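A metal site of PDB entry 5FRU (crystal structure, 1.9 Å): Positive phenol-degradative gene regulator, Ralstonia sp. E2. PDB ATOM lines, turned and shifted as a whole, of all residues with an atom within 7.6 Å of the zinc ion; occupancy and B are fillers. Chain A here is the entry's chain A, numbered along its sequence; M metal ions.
The side-chain carboxylate of Glu 174 lies within hydrogen-bond range of the backbone NH of Val 150 (3.5 Å). SG of Cys 151 sits close to N of Gly 136. SG of Cys 185 sits close to N of Val 178. OG of Ser 133 lies close to SG of Cys 185. O of Cys 185 lies within hydrogen-bond range of N of Trp 130. The side-chain sulfur (SG) of Cys 177 lies close to the backbone NH (N) of Gly 179. SG of Cys 177 lies close to N of Val 150 (3.3 Å).
Four residues have an atom within 4 Å of the zinc ion: Cys 151, Glu 174, Cys 177 and Cys 185.
The zinc ion is bound by OE2 of Glu 174 (2.0 Å), SG of Cys 151 (2.3 Å), SG of Cys 185 (2.4 Å) and SG of Cys 177 (2.4 Å). The zinc ion has four donor atoms within binding distance.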
ATOM      1  N   VAL A 108      10.882  17.083 -16.777  1.00  0.00           N
ATOM      2  CA  VAL A 108      11.383  17.276 -15.438  1.00  0.00           C
ATOM      3  C   VAL A 108      11.278  18.766 -15.113  1.00  0.00           C
ATOM      4  O   VAL A 108      11.222  19.588 -16.018  1.00  0.00           O
ATOM      5  CB  VAL A 108      12.839  16.787 -15.322  1.00  0.00           C
ATOM      6  CG1 VAL A 108      13.766  17.566 -16.289  1.00  0.00           C
ATOM      7  CG2 VAL A 108      13.332  16.838 -13.891  1.00  0.00           C
ATOM      8  N   TRP A 130      16.569  18.291  -9.968  1.00  0.00           N
ATOM      9  CA  TRP A 130      15.460  17.750 -10.772  1.00  0.00           C
ATOM     10  C   TRP A 130      14.275  17.348  -9.907  1.00  0.00           C
ATOM     11  O   TRP A 130      14.419  16.487  -9.052  1.00  0.00           O
ATOM     12  CB  TRP A 130      15.887  16.528 -11.576  1.00  0.00           C
ATOM     13  CG  TRP A 130      16.581  16.832 -12.866  1.00  0.00           C
ATOM     14  CD1 TRP A 130      16.653  18.048 -13.491  1.00  0.00           C
ATOM     15  CD2 TRP A 130      17.313  15.913 -13.682  1.00  0.00           C
ATOM     16  NE1 TRP A 130      17.370  17.929 -14.669  1.00  0.00           N
ATOM     17  CE2 TRP A 130      17.791  16.642 -14.802  1.00  0.00           C
ATOM     18  CE3 TRP A 130      17.600  14.549 -13.586  1.00  0.00           C
ATOM     19  CZ2 TRP A 130      18.546  16.036 -15.823  1.00  0.00           C
ATOM     20  CZ3 TRP A 130      18.367  13.955 -14.589  1.00  0.00           C
ATOM     21  CH2 TRP A 130      18.818  14.706 -15.700  1.00  0.00           C
ATOM     22  N   SER A 133      10.925  14.086 -11.976  1.00  0.00           N
ATOM     23  CA  SER A 133      11.554  13.460 -13.146  1.00  0.00           C
ATOM     24  C   SER A 133      10.623  12.391 -13.712  1.00  0.00           C
ATOM     25  O   SER A 133      10.224  11.479 -12.991  1.00  0.00           O
ATOM     26  CB  SER A 133      12.893  12.815 -12.799  1.00  0.00           C
ATOM     27  OG  SER A 133      13.896  13.793 -12.543  1.00  0.00           O
ATOM     28  N   GLU A 135      11.258  10.102 -15.853  1.00  0.00           N
ATOM     29  CA  GLU A 135      11.945   8.830 -16.081  1.00  0.00           C
ATOM     30  C   GLU A 135      12.095   8.045 -14.784  1.00  0.00           C
ATOM     31  O   GLU A 135      11.886   6.828 -14.756  1.00  0.00           O
ATOM     32  CB  GLU A 135      13.315   9.086 -16.695  1.00  0.00           C
ATOM     33  CG  GLU A 135      13.950   7.856 -17.262  1.00  0.00           C
ATOM     34  CD  GLU A 135      15.087   8.169 -18.209  1.00  0.00           C
ATOM     35  OE1 GLU A 135      15.531   9.337 -18.251  1.00  0.00           O
ATOM     36  OE2 GLU A 135      15.561   7.235 -18.912  1.00  0.00           O
ATOM     37  N   GLY A 136      12.455   8.731 -13.716  1.00  0.00           N
ATOM     38  CA  GLY A 136      12.683   8.040 -12.451  1.00  0.00           C
ATOM     39  C   GLY A 136      11.368   7.460 -11.972  1.00  0.00           C
ATOM     40  O   GLY A 136      11.304   6.319 -11.483  1.00  0.00           O
ATOM     41  N   ASP A 137      10.312   8.235 -12.141  1.00  0.00           N
ATOM     42  CA  ASP A 137       8.991   7.791 -11.739  1.00  0.00           C
ATOM     43  C   ASP A 137       8.564   6.587 -12.596  1.00  0.00           C
ATOM     44  O   ASP A 137       8.099   5.585 -12.058  1.00  0.00           O
ATOM     45  CB  ASP A 137       7.985   8.943 -11.835  1.00  0.00           C
ATOM     46  CG  ASP A 137       8.420  10.177 -11.021  1.00  0.00           C
ATOM     47  OD1 ASP A 137       9.543  10.197 -10.474  1.00  0.00           O
ATOM     48  OD2 ASP A 137       7.620  11.148 -10.948  1.00  0.00           O
ATOM     49  N   ALA A 148      20.698   2.130  -8.380  1.00  0.00           N
ATOM     50  CA  ALA A 148      21.561   3.211  -8.863  1.00  0.00           C
ATOM     51  C   ALA A 148      20.675   4.228  -9.601  1.00  0.00           C
ATOM     52  O   ALA A 148      19.533   3.922  -9.902  1.00  0.00           O
ATOM     53  CB  ALA A 148      22.639   2.662  -9.774  1.00  0.00           C
ATOM     54  N   PRO A 149      21.164   5.458  -9.823  1.00  0.00           N
ATOM     55  CA  PRO A 149      20.320   6.452 -10.523  1.00  0.00           C
ATOM     56  C   PRO A 149      19.805   5.926 -11.871  1.00  0.00           C
ATOM     57  O   PRO A 149      20.472   5.130 -12.504  1.00  0.00           O
ATOM     58  CB  PRO A 149      21.274   7.630 -10.737  1.00  0.00           C
ATOM     59  CG  PRO A 149      22.204   7.541  -9.566  1.00  0.00           C
ATOM     60  CD  PRO A 149      22.422   6.060  -9.327  1.00  0.00           C
ATOM     61  N   VAL A 150      18.624   6.347 -12.298  1.00  0.00           N
ATOM     62  CA  VAL A 150      18.080   5.740 -13.514  1.00  0.00           C
ATOM     63  C   VAL A 150      17.519   6.696 -14.568  1.00  0.00           C
ATOM     64  O   VAL A 150      16.884   6.246 -15.529  1.00  0.00           O
ATOM     65  CB  VAL A 150      16.993   4.711 -13.158  1.00  0.00           C
ATOM     66  CG1 VAL A 150      17.630   3.483 -12.548  1.00  0.00           C
ATOM     67  CG2 VAL A 150      15.994   5.300 -12.196  1.00  0.00           C
ATOM     68  N   CYS A 151      17.755   7.996 -14.444  1.00  0.00           N
ATOM     69  CA  CYS A 151      17.192   8.930 -15.425  1.00  0.00           C
ATOM     70  C   CYS A 151      18.118   9.013 -16.651  1.00  0.00           C
ATOM     71  O   CYS A 151      18.701  10.046 -16.984  1.00  0.00           O
ATOM     72  CB  CYS A 151      16.939  10.295 -14.786  1.00  0.00           C
ATOM     73  SG  CYS A 151      15.608  10.202 -13.516  1.00  0.00           S
ATOM     74  N   TRP A 152      18.222   7.871 -17.328  1.00  0.00           N
ATOM     75  CA  TRP A 152      19.135   7.690 -18.445  1.00  0.00           C
ATOM     76  C   TRP A 152      18.876   8.692 -19.582  1.00  0.00           C
ATOM     77  O   TRP A 152      19.804   9.386 -20.028  1.00  0.00           O
ATOM     78  CB  TRP A 152      19.035   6.268 -18.964  1.00  0.00           C
ATOM     79  CG  TRP A 152      19.201   5.206 -17.914  1.00  0.00           C
ATOM     80  CD1 TRP A 152      19.995   5.261 -16.800  1.00  0.00           C
ATOM     81  CD2 TRP A 152      18.562   3.924 -17.888  1.00  0.00           C
ATOM     82  NE1 TRP A 152      19.890   4.095 -16.078  1.00  0.00           N
ATOM     83  CE2 TRP A 152      19.003   3.263 -16.722  1.00  0.00           C
ATOM     84  CE3 TRP A 152      17.647   3.280 -18.726  1.00  0.00           C
ATOM     85  CZ2 TRP A 152      18.581   1.975 -16.387  1.00  0.00           C
ATOM     86  CZ3 TRP A 152      17.213   1.998 -18.387  1.00  0.00           C
ATOM     87  CH2 TRP A 152      17.688   1.360 -17.230  1.00  0.00           C
ATOM     88  N   GLN A 154      17.145  11.410 -19.511  1.00  0.00           N
ATOM     89  CA  GLN A 154      17.248  12.786 -19.037  1.00  0.00           C
ATOM     90  C   GLN A 154      18.706  13.222 -18.927  1.00  0.00           C
ATOM     91  O   GLN A 154      19.044  14.354 -19.251  1.00  0.00           O
ATOM     92  CB  GLN A 154      16.547  12.958 -17.673  1.00  0.00           C
ATOM     93  CG  GLN A 154      15.056  12.653 -17.736  1.00  0.00           C
ATOM     94  CD  GLN A 154      14.318  12.829 -16.413  1.00  0.00           C
ATOM     95  OE1 GLN A 154      13.220  12.333 -16.251  1.00  0.00           O
ATOM     96  NE2 GLN A 154      14.931  13.539 -15.466  1.00  0.00           N
ATOM     97  N   ILE A 155      19.573  12.315 -18.483  1.00  0.00           N
ATOM     98  CA  ILE A 155      20.998  12.605 -18.399  1.00  0.00           C
ATOM     99  C   ILE A 155      21.556  12.746 -19.821  1.00  0.00           C
ATOM    100  O   ILE A 155      22.384  13.616 -20.091  1.00  0.00           O
ATOM    101  CB  ILE A 155      21.766  11.504 -17.638  1.00  0.00           C
ATOM    102  CG1 ILE A 155      21.518  11.621 -16.126  1.00  0.00           C
ATOM    103  CG2 ILE A 155      23.252  11.570 -17.918  1.00  0.00           C
ATOM    104  CD1 ILE A 155      22.101  12.898 -15.504  1.00  0.00           C
ATOM    105  N   GLU A 174      24.052  11.619 -12.301  1.00  0.00           N
ATOM    106  CA  GLU A 174      23.154  11.901 -11.195  1.00  0.00           C
ATOM    107  C   GLU A 174      23.823  11.599  -9.866  1.00  0.00           C
ATOM    108  O   GLU A 174      24.431  10.554  -9.712  1.00  0.00           O
ATOM    109  CB  GLU A 174      21.858  11.084 -11.309  1.00  0.00           C
ATOM    110  CG  GLU A 174      20.898  11.601 -12.348  1.00  0.00           C
ATOM    111  CD  GLU A 174      19.635  10.797 -12.410  1.00  0.00           C
ATOM    112  OE1 GLU A 174      19.688   9.612 -12.831  1.00  0.00           O
ATOM    113  OE2 GLU A 174      18.587  11.359 -12.043  1.00  0.00           O
ATOM    114  N   GLU A 176      22.001  12.006  -6.907  1.00  0.00           N
ATOM    115  CA  GLU A 176      20.880  11.320  -6.284  1.00  0.00           C
ATOM    116  C   GLU A 176      19.718  11.255  -7.272  1.00  0.00           C
ATOM    117  O   GLU A 176      19.708  11.967  -8.269  1.00  0.00           O
ATOM    118  CB  GLU A 176      20.462  12.018  -4.989  1.00  0.00           C
ATOM    119  CG  GLU A 176      19.931  13.436  -5.131  1.00  0.00           C
ATOM    120  CD  GLU A 176      19.658  14.075  -3.759  1.00  0.00           C
ATOM    121  OE1 GLU A 176      19.527  13.327  -2.760  1.00  0.00           O
ATOM    122  OE2 GLU A 176      19.578  15.321  -3.683  1.00  0.00           O
ATOM    123  N   CYS A 177      18.730  10.398  -7.003  1.00  0.00           N
ATOM    124  CA  CYS A 177      17.723  10.109  -8.007  1.00  0.00           C
ATOM    125  C   CYS A 177      16.442   9.561  -7.380  1.00  0.00           C
ATOM    126  O   CYS A 177      16.486   8.686  -6.505  1.00  0.00           O
ATOM    127  CB  CYS A 177      18.290   9.103  -9.036  1.00  0.00           C
ATOM    128  SG  CYS A 177      17.100   8.585 -10.337  1.00  0.00           S
ATOM    129  N   VAL A 178      15.305  10.093  -7.816  1.00  0.00           N
ATOM    130  CA  VAL A 178      14.023   9.622  -7.354  1.00  0.00           C
ATOM    131  C   VAL A 178      13.837   8.158  -7.699  1.00  0.00           C
ATOM    132  O   VAL A 178      13.087   7.446  -7.017  1.00  0.00           O
ATOM    133  CB  VAL A 178      12.858  10.433  -7.948  1.00  0.00           C
ATOM    134  CG1 VAL A 178      12.886  11.833  -7.439  1.00  0.00           C
ATOM    135  CG2 VAL A 178      12.905  10.393  -9.487  1.00  0.00           C
ATOM    136  N   GLY A 179      14.534   7.694  -8.738  1.00  0.00           N
ATOM    137  CA  GLY A 179      14.392   6.309  -9.168  1.00  0.00           C
ATOM    138  C   GLY A 179      14.988   5.358  -8.136  1.00  0.00           C
ATOM    139  O   GLY A 179      14.698   4.160  -8.134  1.00  0.00           O
ATOM    140  N   CYS A 180      15.825   5.930  -7.276  1.00  0.00           N
ATOM    141  CA  CYS A 180      16.499   5.239  -6.185  1.00  0.00           C
ATOM    142  C   CYS A 180      15.785   5.380  -4.860  1.00  0.00           C
ATOM    143  O   CYS A 180      16.304   4.944  -3.824  1.00  0.00           O
ATOM    144  CB  CYS A 180      17.902   5.781  -5.979  1.00  0.00           C
ATOM    145  SG  CYS A 180      19.011   5.498  -7.267  1.00  0.00           S
ATOM    146  N   HIS A 184      14.294  13.822  -4.657  1.00  0.00           N
ATOM    147  CA  HIS A 184      14.613  14.432  -5.972  1.00  0.00           C
ATOM    148  C   HIS A 184      15.770  13.760  -6.661  1.00  0.00           C
ATOM    149  O   HIS A 184      16.401  12.871  -6.131  1.00  0.00           O
ATOM    150  CB  HIS A 184      15.028  15.929  -5.929  1.00  0.00           C
ATOM    151  CG  HIS A 184      14.000  16.850  -5.355  1.00  0.00           C
ATOM    152  ND1 HIS A 184      12.816  17.131  -5.996  1.00  0.00           N
ATOM    153  CD2 HIS A 184      13.783  17.211  -4.064  1.00  0.00           C
ATOM    154  CE1 HIS A 184      12.054  17.878  -5.230  1.00  0.00           C
ATOM    155  NE2 HIS A 184      12.613  17.919  -4.031  1.00  0.00           N
ATOM    156  N   CYS A 185      16.088  14.307  -7.833  1.00  0.00           N
ATOM    157  CA  CYS A 185      17.319  14.018  -8.509  1.00  0.00           C
ATOM    158  C   CYS A 185      18.203  15.255  -8.405  1.00  0.00           C
ATOM    159  O   CYS A 185      17.728  16.382  -8.313  1.00  0.00           O
ATOM    160  CB  CYS A 185      17.117  13.667 -10.002  1.00  0.00           C
ATOM    161  SG  CYS A 185      15.892  12.384 -10.336  1.00  0.00           S
ATOM    162  N   ARG A 186      19.501  15.012  -8.438  1.00  0.00           N
ATOM    163  CA  ARG A 186      20.494  16.090  -8.459  1.00  0.00           C
ATOM    164  C   ARG A 186      21.565  15.686  -9.435  1.00  0.00           C
ATOM    165  O   ARG A 186      22.022  14.534  -9.396  1.00  0.00           O
ATOM    166  CB  ARG A 186      21.028  16.306  -7.056  1.00  0.00           C
ATOM    167  CG  ARG A 186      22.043  17.400  -6.914  1.00  0.00           C
ATOM    168  CD  ARG A 186      22.418  17.538  -5.474  1.00  0.00           C
ATOM    169  NE  ARG A 186      23.096  16.349  -4.971  1.00  0.00           N
ATOM    170  CZ  ARG A 186      24.393  16.124  -5.130  1.00  0.00           C
ATOM    171  NH1 ARG A 186      25.145  17.012  -5.774  1.00  0.00           N
ATOM    172  NH2 ARG A 186      24.936  15.012  -4.654  1.00  0.00           N
ATOM    173  N   ILE A 187      21.970  16.583 -10.337  1.00  0.00           N
ATOM    174  CA  ILE A 187      22.941  16.205 -11.354  1.00  0.00           C
ATOM    175  C   ILE A 187      24.146  17.138 -11.364  1.00  0.00           C
ATOM    176  O   ILE A 187      24.066  18.277 -10.904  1.00  0.00           O
ATOM    177  CB  ILE A 187      22.339  16.192 -12.770  1.00  0.00           C
ATOM    178  CG1 ILE A 187      22.040  17.615 -13.237  1.00  0.00           C
ATOM    179  CG2 ILE A 187      21.089  15.287 -12.839  1.00  0.00           C
ATOM    180  CD1 ILE A 187      21.293  17.688 -14.551  1.00  0.00           C
HETATM  181 ZN    ZN M   1      16.821  10.591 -11.565  1.00  0.00          ZN
